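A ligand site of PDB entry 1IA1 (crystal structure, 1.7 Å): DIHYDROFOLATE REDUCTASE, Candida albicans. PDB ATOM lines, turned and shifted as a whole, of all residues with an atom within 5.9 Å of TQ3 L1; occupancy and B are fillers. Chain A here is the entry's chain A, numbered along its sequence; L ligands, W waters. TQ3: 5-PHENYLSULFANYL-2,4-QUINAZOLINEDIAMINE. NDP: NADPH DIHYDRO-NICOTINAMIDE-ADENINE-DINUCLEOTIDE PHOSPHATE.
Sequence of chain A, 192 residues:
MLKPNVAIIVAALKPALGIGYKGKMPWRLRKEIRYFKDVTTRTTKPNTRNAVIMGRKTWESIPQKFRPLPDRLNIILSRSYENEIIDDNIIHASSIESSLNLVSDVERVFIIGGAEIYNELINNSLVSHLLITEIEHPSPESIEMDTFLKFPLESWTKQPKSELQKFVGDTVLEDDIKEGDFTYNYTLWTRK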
ATOM      1  N   ILE A   9      34.851  12.338  17.970  1.00  0.00           N
ATOM      2  CA  ILE A   9      34.283  12.950  19.218  1.00  0.00           C
ATOM      3  C   ILE A   9      32.799  12.623  19.162  1.00  0.00           C
ATOM      4  O   ILE A   9      32.127  12.939  18.192  1.00  0.00           O
ATOM      5  CB  ILE A   9      34.615  14.438  19.369  1.00  0.00           C
ATOM      6  CG1 ILE A   9      33.937  15.026  20.680  1.00  0.00           C
ATOM      7  CG2 ILE A   9      34.139  15.288  18.156  1.00  0.00           C
ATOM      8  CD1 ILE A   9      34.724  16.354  21.123  1.00  0.00           C
ATOM      9  N   VAL A  10      32.316  12.024  20.281  1.00  0.00           N
ATOM     10  CA  VAL A  10      30.894  11.604  20.368  1.00  0.00           C
ATOM     11  C   VAL A  10      30.425  11.584  21.825  1.00  0.00           C
ATOM     12  O   VAL A  10      31.287  11.413  22.724  1.00  0.00           O
ATOM     13  CB  VAL A  10      30.782  10.191  19.722  1.00  0.00           C
ATOM     14  CG1 VAL A  10      31.666   9.152  20.494  1.00  0.00           C
ATOM     15  CG2 VAL A  10      29.363   9.677  19.642  1.00  0.00           C
ATOM     16  N   ALA A  11      29.124  11.711  21.982  1.00  0.00           N
ATOM     17  CA  ALA A  11      28.502  11.541  23.353  1.00  0.00           C
ATOM     18  C   ALA A  11      27.612  10.303  23.307  1.00  0.00           C
ATOM     19  O   ALA A  11      26.776  10.169  22.407  1.00  0.00           O
ATOM     20  CB  ALA A  11      27.727  12.807  23.697  1.00  0.00           C
ATOM     21  N   MET A  25      19.457  13.974  18.868  1.00  0.00           N
ATOM     22  CA  MET A  25      20.145  13.463  20.095  1.00  0.00           C
ATOM     23  C   MET A  25      19.020  13.332  21.142  1.00  0.00           C
ATOM     24  O   MET A  25      18.093  14.159  21.193  1.00  0.00           O
ATOM     25  CB  MET A  25      21.328  14.295  20.539  1.00  0.00           C
ATOM     26  CG  MET A  25      22.450  14.212  19.537  1.00  0.00           C
ATOM     27  SD  MET A  25      23.721  15.476  19.877  1.00  0.00           S
ATOM     28  CE  MET A  25      24.417  14.803  21.412  1.00  0.00           C
ATOM     29  N   GLU A  32      27.924  19.849  28.082  1.00  0.00           N
ATOM     30  CA  GLU A  32      28.620  18.926  27.086  1.00  0.00           C
ATOM     31  C   GLU A  32      28.739  19.606  25.761  1.00  0.00           C
ATOM     32  O   GLU A  32      29.811  19.497  25.124  1.00  0.00           O
ATOM     33  CB  GLU A  32      27.768  17.663  26.968  1.00  0.00           C
ATOM     34  CG  GLU A  32      28.550  16.357  26.630  1.00  0.00           C
ATOM     35  CD  GLU A  32      29.024  16.289  25.199  1.00  0.00           C
ATOM     36  OE1 GLU A  32      28.332  16.751  24.319  1.00  0.00           O
ATOM     37  OE2 GLU A  32      30.127  15.700  24.993  1.00  0.00           O
ATOM     38  N   ILE A  33      27.675  20.287  25.324  1.00  0.00           N
ATOM     39  CA  ILE A  33      27.713  21.055  24.106  1.00  0.00           C
ATOM     40  C   ILE A  33      28.842  22.095  24.164  1.00  0.00           C
ATOM     41  O   ILE A  33      29.507  22.288  23.158  1.00  0.00           O
ATOM     42  CB  ILE A  33      26.336  21.807  23.778  1.00  0.00           C
ATOM     43  CG1 ILE A  33      25.189  20.852  23.771  1.00  0.00           C
ATOM     44  CG2 ILE A  33      26.480  22.676  22.498  1.00  0.00           C
ATOM     45  CD1 ILE A  33      25.013  19.662  22.927  1.00  0.00           C
ATOM     46  N   TYR A  35      31.654  21.990  25.890  1.00  0.00           N
ATOM     47  CA  TYR A  35      32.918  21.219  25.811  1.00  0.00           C
ATOM     48  C   TYR A  35      33.176  20.900  24.318  1.00  0.00           C
ATOM     49  O   TYR A  35      34.298  21.096  23.854  1.00  0.00           O
ATOM     50  CB  TYR A  35      32.780  19.920  26.606  1.00  0.00           C
ATOM     51  CG  TYR A  35      33.810  18.850  26.363  1.00  0.00           C
ATOM     52  CD1 TYR A  35      33.588  17.749  25.487  1.00  0.00           C
ATOM     53  CD2 TYR A  35      35.040  18.939  27.011  1.00  0.00           C
ATOM     54  CE1 TYR A  35      34.604  16.801  25.300  1.00  0.00           C
ATOM     55  CE2 TYR A  35      36.034  17.995  26.841  1.00  0.00           C
ATOM     56  CZ  TYR A  35      35.795  16.931  25.981  1.00  0.00           C
ATOM     57  OH  TYR A  35      36.850  16.020  25.915  1.00  0.00           O
ATOM     58  N   PHE A  36      32.175  20.337  23.685  1.00  0.00           N
ATOM     59  CA  PHE A  36      32.284  19.995  22.218  1.00  0.00           C
ATOM     60  C   PHE A  36      32.821  21.215  21.469  1.00  0.00           C
ATOM     61  O   PHE A  36      33.758  21.105  20.652  1.00  0.00           O
ATOM     62  CB  PHE A  36      31.009  19.407  21.684  1.00  0.00           C
ATOM     63  CG  PHE A  36      30.922  19.362  20.190  1.00  0.00           C
ATOM     64  CD1 PHE A  36      30.231  20.386  19.512  1.00  0.00           C
ATOM     65  CD2 PHE A  36      31.612  18.358  19.467  1.00  0.00           C
ATOM     66  CE1 PHE A  36      30.181  20.391  18.122  1.00  0.00           C
ATOM     67  CE2 PHE A  36      31.543  18.365  18.062  1.00  0.00           C
ATOM     68  CZ  PHE A  36      30.878  19.406  17.413  1.00  0.00           C
ATOM     69  N   MET A  54      31.620  15.604   8.874  1.00  0.00           N
ATOM     70  CA  MET A  54      30.333  14.995   9.262  1.00  0.00           C
ATOM     71  C   MET A  54      29.666  14.343   8.041  1.00  0.00           C
ATOM     72  O   MET A  54      29.985  14.834   6.916  1.00  0.00           O
ATOM     73  CB  MET A  54      29.437  16.084   9.905  1.00  0.00           C
ATOM     74  CG  MET A  54      28.963  17.104   8.905  1.00  0.00           C
ATOM     75  SD  MET A  54      28.332  18.578   9.800  1.00  0.00           S
ATOM     76  CE  MET A  54      29.751  19.646   9.607  1.00  0.00           C
ATOM     77  N   THR A  58      23.786  14.558   9.095  1.00  0.00           N
ATOM     78  CA  THR A  58      24.121  15.431  10.241  1.00  0.00           C
ATOM     79  C   THR A  58      24.125  16.889   9.789  1.00  0.00           C
ATOM     80  O   THR A  58      23.516  17.744  10.443  1.00  0.00           O
ATOM     81  CB  THR A  58      25.375  14.975  11.021  1.00  0.00           C
ATOM     82  OG1 THR A  58      25.024  13.663  11.590  1.00  0.00           O
ATOM     83  CG2 THR A  58      25.723  15.940  12.195  1.00  0.00           C
ATOM     84  N   SER A  61      20.759  18.293   9.387  1.00  0.00           N
ATOM     85  CA  SER A  61      20.031  18.451  10.642  1.00  0.00           C
ATOM     86  C   SER A  61      20.310  19.792  11.261  1.00  0.00           C
ATOM     87  O   SER A  61      19.537  20.148  12.201  1.00  0.00           O
ATOM     88  CB  SER A  61      20.321  17.281  11.596  1.00  0.00           C
ATOM     89  OG  SER A  61      21.568  17.436  12.285  1.00  0.00           O
ATOM     90  N   ILE A  62      21.343  20.514  10.852  1.00  0.00           N
ATOM     91  CA  ILE A  62      21.613  21.848  11.483  1.00  0.00           C
ATOM     92  C   ILE A  62      20.710  22.829  10.711  1.00  0.00           C
ATOM     93  O   ILE A  62      20.699  22.815   9.464  1.00  0.00           O
ATOM     94  CB  ILE A  62      23.116  22.240  11.275  1.00  0.00           C
ATOM     95  CG1 ILE A  62      24.061  21.080  11.821  1.00  0.00           C
ATOM     96  CG2 ILE A  62      23.486  23.573  11.941  1.00  0.00           C
ATOM     97  CD1 ILE A  62      25.526  21.236  11.337  1.00  0.00           C
ATOM     98  N   LEU A  69      29.342  25.311  10.900  1.00  0.00           N
ATOM     99  CA  LEU A  69      29.725  25.583  12.345  1.00  0.00           C
ATOM    100  C   LEU A  69      30.838  26.627  12.290  1.00  0.00           C
ATOM    101  O   LEU A  69      31.821  26.531  11.538  1.00  0.00           O
ATOM    102  CB  LEU A  69      30.099  24.249  12.963  1.00  0.00           C
ATOM    103  CG  LEU A  69      29.045  23.202  13.091  1.00  0.00           C
ATOM    104  CD1 LEU A  69      29.623  21.911  13.758  1.00  0.00           C
ATOM    105  CD2 LEU A  69      27.830  23.617  13.879  1.00  0.00           C
ATOM    106  N   ILE A 111      36.126  13.898  13.604  1.00  0.00           N
ATOM    107  CA  ILE A 111      34.899  13.343  12.975  1.00  0.00           C
ATOM    108  C   ILE A 111      33.758  13.567  14.057  1.00  0.00           C
ATOM    109  O   ILE A 111      33.942  13.058  15.150  1.00  0.00           O
ATOM    110  CB  ILE A 111      35.065  11.826  12.720  1.00  0.00           C
ATOM    111  CG1 ILE A 111      36.111  11.706  11.507  1.00  0.00           C
ATOM    112  CG2 ILE A 111      33.734  11.129  12.312  1.00  0.00           C
ATOM    113  CD1 ILE A 111      36.675  10.250  11.468  1.00  0.00           C
ATOM    114  N   ILE A 112      32.728  14.282  13.610  1.00  0.00           N
ATOM    115  CA  ILE A 112      31.671  14.628  14.586  1.00  0.00           C
ATOM    116  C   ILE A 112      30.361  13.923  14.456  1.00  0.00           C
ATOM    117  O   ILE A 112      29.417  14.194  15.216  1.00  0.00           O
ATOM    118  CB  ILE A 112      31.552  16.214  14.601  1.00  0.00           C
ATOM    119  CG1 ILE A 112      30.900  16.713  13.307  1.00  0.00           C
ATOM    120  CG2 ILE A 112      32.907  16.838  15.009  1.00  0.00           C
ATOM    121  CD1 ILE A 112      30.339  18.150  13.354  1.00  0.00           C
ATOM    122  N   GLY A 113      30.288  12.969  13.505  1.00  0.00           N
ATOM    123  CA  GLY A 113      29.090  12.160  13.322  1.00  0.00           C
ATOM    124  C   GLY A 113      28.550  12.175  11.937  1.00  0.00           C
ATOM    125  O   GLY A 113      29.074  12.837  11.025  1.00  0.00           O
ATOM    126  N   TYR A 118      30.385   7.340  11.932  1.00  0.00           N
ATOM    127  CA  TYR A 118      31.170   6.768  13.032  1.00  0.00           C
ATOM    128  C   TYR A 118      31.443   5.263  12.839  1.00  0.00           C
ATOM    129  O   TYR A 118      32.591   4.874  13.153  1.00  0.00           O
ATOM    130  CB  TYR A 118      30.454   6.886  14.392  1.00  0.00           C
ATOM    131  CG  TYR A 118      30.309   8.277  14.985  1.00  0.00           C
ATOM    132  CD1 TYR A 118      31.408   9.129  15.128  1.00  0.00           C
ATOM    133  CD2 TYR A 118      29.085   8.619  15.531  1.00  0.00           C
ATOM    134  CE1 TYR A 118      31.259  10.362  15.765  1.00  0.00           C
ATOM    135  CE2 TYR A 118      28.907   9.841  16.179  1.00  0.00           C
ATOM    136  CZ  TYR A 118      29.987  10.694  16.308  1.00  0.00           C
ATOM    137  OH  TYR A 118      29.846  11.890  16.907  1.00  0.00           O
ATOM    138  N   LEU A 131      37.392  10.502  21.505  1.00  0.00           N
ATOM    139  CA  LEU A 131      36.946  11.363  22.643  1.00  0.00           C
ATOM    140  C   LEU A 131      35.480  10.997  22.822  1.00  0.00           C
ATOM    141  O   LEU A 131      34.604  11.489  22.082  1.00  0.00           O
ATOM    142  CB  LEU A 131      37.217  12.829  22.359  1.00  0.00           C
ATOM    143  CG  LEU A 131      38.606  13.399  22.402  1.00  0.00           C
ATOM    144  CD1 LEU A 131      38.625  14.882  21.974  1.00  0.00           C
ATOM    145  CD2 LEU A 131      39.242  13.303  23.767  1.00  0.00           C
ATOM    146  N   THR A 133      32.273  11.041  25.299  1.00  0.00           N
ATOM    147  CA  THR A 133      31.618  11.505  26.621  1.00  0.00           C
ATOM    148  C   THR A 133      30.744  10.301  27.053  1.00  0.00           C
ATOM    149  O   THR A 133      29.814   9.866  26.332  1.00  0.00           O
ATOM    150  CB  THR A 133      30.721  12.782  26.402  1.00  0.00           C
ATOM    151  OG1 THR A 133      31.654  13.829  25.966  1.00  0.00           O
ATOM    152  CG2 THR A 133      30.012  13.205  27.724  1.00  0.00           C
HETATM  153  C1  TQ3 L   1      28.305  16.849  20.846  1.00  0.00           C
HETATM  154  C2  TQ3 L   1      28.550  16.519  19.508  1.00  0.00           C
HETATM  155  C3  TQ3 L   1      29.635  15.537  19.267  1.00  0.00           C
HETATM  156  N4  TQ3 L   1      30.313  15.017  20.247  1.00  0.00           N
HETATM  157  C5  TQ3 L   1      30.162  15.409  21.514  1.00  0.00           C
HETATM  158  N6  TQ3 L   1      29.101  16.233  21.889  1.00  0.00           N
HETATM  159  N7  TQ3 L   1      29.957  15.080  18.089  1.00  0.00           N
HETATM  160  C8  TQ3 L   1      27.296  17.729  21.203  1.00  0.00           C
HETATM  161  C9  TQ3 L   1      26.504  18.322  20.180  1.00  0.00           C
HETATM  162  C12 TQ3 L   1      26.741  18.037  18.823  1.00  0.00           C
HETATM  163  C13 TQ3 L   1      27.750  17.151  18.501  1.00  0.00           C
HETATM  164  N14 TQ3 L   1      30.815  14.904  22.539  1.00  0.00           N
HETATM  165  S20 TQ3 L   1      28.041  16.876  16.765  1.00  0.00           S
HETATM  166  C22 TQ3 L   1      26.561  17.516  15.938  1.00  0.00           C
HETATM  167  C23 TQ3 L   1      25.341  16.877  16.052  1.00  0.00           C
HETATM  168  C24 TQ3 L   1      24.217  17.378  15.378  1.00  0.00           C
HETATM  169  C25 TQ3 L   1      24.376  18.514  14.555  1.00  0.00           C
HETATM  170  C26 TQ3 L   1      25.608  19.149  14.400  1.00  0.00           C
HETATM  171  C27 TQ3 L   1      26.740  18.657  15.093  1.00  0.00           C
HETATM  172  PA  NDP L   2      25.182  10.605   9.132  1.00  0.00           P
HETATM  173  O1A NDP L   2      26.145   9.585   9.589  1.00  0.00           O
HETATM  174  O2A NDP L   2      25.442  11.954   9.701  1.00  0.00           O
HETATM  175  O5B NDP L   2      25.049  10.721   7.544  1.00  0.00           O
HETATM  176  C5B NDP L   2      24.967   9.510   6.742  1.00  0.00           C
HETATM  177  C4B NDP L   2      25.278   9.941   5.303  1.00  0.00           C
HETATM  178  O4B NDP L   2      26.671  10.253   5.181  1.00  0.00           O
HETATM  179  C3B NDP L   2      25.061   8.792   4.263  1.00  0.00           C
HETATM  180  O3B NDP L   2      23.672   8.786   3.921  1.00  0.00           O
HETATM  181  C2B NDP L   2      26.050   9.299   3.121  1.00  0.00           C
HETATM  182  O2B NDP L   2      25.526  10.469   2.434  1.00  0.00           O
HETATM  183  C1B NDP L   2      27.190   9.843   3.962  1.00  0.00           C
HETATM  184  N9A NDP L   2      28.173   8.861   4.243  1.00  0.00           N
HETATM  185  C8A NDP L   2      28.076   7.915   5.201  1.00  0.00           C
HETATM  186  N7A NDP L   2      29.136   7.121   5.249  1.00  0.00           N
HETATM  187  C5A NDP L   2      29.923   7.587   4.243  1.00  0.00           C
HETATM  188  C6A NDP L   2      31.191   7.147   3.808  1.00  0.00           C
HETATM  189  N6A NDP L   2      31.789   6.093   4.402  1.00  0.00           N
HETATM  190  N1A NDP L   2      31.739   7.854   2.838  1.00  0.00           N
HETATM  191  C2A NDP L   2      31.065   8.881   2.236  1.00  0.00           C
HETATM  192  N3A NDP L   2      29.878   9.347   2.571  1.00  0.00           N
HETATM  193  C4A NDP L   2      29.371   8.675   3.608  1.00  0.00           C
HETATM  194  O3  NDP L   2      23.769  10.128   9.516  1.00  0.00           O
HETATM  195  PN  NDP L   2      23.009   9.040  10.403  1.00  0.00           P
HETATM  196  O1N NDP L   2      21.576   9.084  10.165  1.00  0.00           O
HETATM  197  O2N NDP L   2      23.655   7.704  10.302  1.00  0.00           O
HETATM  198  O5D NDP L   2      23.295   9.549  11.923  1.00  0.00           O
HETATM  199  C5D NDP L   2      22.382  10.522  12.481  1.00  0.00           C
HETATM  200  C4D NDP L   2      22.191  10.202  13.953  1.00  0.00           C
HETATM  201  O4D NDP L   2      23.445  10.369  14.670  1.00  0.00           O
HETATM  202  C3D NDP L   2      21.171  11.184  14.626  1.00  0.00           C
HETATM  203  O3D NDP L   2      20.344  10.408  15.495  1.00  0.00           O
HETATM  204  C2D NDP L   2      22.149  12.146  15.297  1.00  0.00           C
HETATM  205  O2D NDP L   2      21.532  12.769  16.438  1.00  0.00           O
HETATM  206  C1D NDP L   2      23.259  11.208  15.759  1.00  0.00           C
HETATM  207  N1N NDP L   2      24.491  11.949  16.181  1.00  0.00           N
HETATM  208  C2N NDP L   2      24.845  11.735  17.508  1.00  0.00           C
HETATM  209  C3N NDP L   2      25.907  12.440  18.012  1.00  0.00           C
HETATM  210  C7N NDP L   2      26.271  12.194  19.517  1.00  0.00           C
HETATM  211  O7N NDP L   2      27.345  12.696  19.878  1.00  0.00           O
HETATM  212  N7N NDP L   2      25.488  11.424  20.280  1.00  0.00           N
HETATM  213  C4N NDP L   2      26.770  13.276  17.242  1.00  0.00           C
HETATM  214  C5N NDP L   2      26.298  13.413  15.911  1.00  0.00           C
HETATM  215  C6N NDP L   2      25.220  12.810  15.341  1.00  0.00           C
HETATM  216  P2B NDP L   2      24.750  10.070   0.976  1.00  0.00           P
HETATM  217  O1X NDP L   2      24.511  11.479   0.451  1.00  0.00           O
HETATM  218  O2X NDP L   2      25.780   9.246   0.358  1.00  0.00           O
HETATM  219  O3X NDP L   2      23.546   9.375   1.463  1.00  0.00           O
HETATM  220  O   HOH W   1      33.636  13.579  24.043  1.00  0.00           O
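A nitrogen (N6) of TQ3 L1 sits at hydrogen-bond distance from the side-chain carboxylate (OE1) of Glu 32 (2.6 Å).
The backbone carbonyl oxygen (O) of Ile 9 is in hydrogen-bond range of a nitrogen (N7) of TQ3 L1 (3.1 Å).
The backbone carbonyl oxygen (O) of Ile 112 is in hydrogen-bond range of a nitrogen (N7) of TQ3 L1, 3.1 Å away.
OH of Tyr 118 lies within hydrogen-bond range of N7 of TQ3 L1, at 3.4 Å.
The backbone NH (N) of Ala 11 is in hydrogen-bond range of an oxygen (O7N) of NDP L2, at 2.9 Å.
O of Ala 11 lies within hydrogen-bond range of N7N of NDP L2 (2.8 Å).
O2A of NDP L2 lies within hydrogen-bond range of N of Thr 58 (3.1 Å).
An oxygen (O2A) of NDP L2 is in hydrogen-bond range of the side-chain hydroxyl (OG1) of Thr 58 (2.6 Å).
N of Met 25 lies within hydrogen-bond range of O2D of NDP L2 (3.4 Å).
OG1 of Thr 133 is in hydrogen-bond range of OE2 of Glu 32 (2.6 Å).
The backbone carbonyl oxygen (O) of Ile 9 is in hydrogen-bond range of the side-chain hydroxyl (OH) of Tyr 118 (2.8 Å).
N of Ile 9 sits at hydrogen-bond distance from O of Ile 111, 3.0 Å away.
O of Ile 112 lies within hydrogen-bond range of OH of Tyr 118, 2.9 Å away.
O of Val 10 sits at hydrogen-bond distance from N of Thr 133, 2.8 Å away.
The backbone NH (N) of Val 10 lies within hydrogen-bond range of the backbone carbonyl oxygen (O) of Leu 131, 3.0 Å away.
The backbone carbonyl oxygen (O) of Thr 58 sits at hydrogen-bond distance from the side-chain hydroxyl (OG) of Ser 61 (2.7 Å).
Merely in contact with TQ3 L1: Val 10 (3.4 Å), Ala 11 (3.7 Å), Met 25 (3.99 Å), Ile 33 (3.4 Å), Phe 36 (3.5 Å), Thr 58 (3.7 Å), Ser 61 (3.8 Å), Ile 62 (3.6 Å) and Thr 133 (3.7 Å).
Of the 19 residues printed, 13 come within 4 Å of TQ3 L1.
Along chain A the residues within 4 Å of TQ3 L1 span positions 9 to 133.
The nearest printed residue that does not touch TQ3 L1 is Leu 69 (4.5 Å).
Water W1 lies within hydrogen-bond range of OG1 of Thr 133, O of Leu 131, O of Val 10 and N14 of TQ3 L1.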
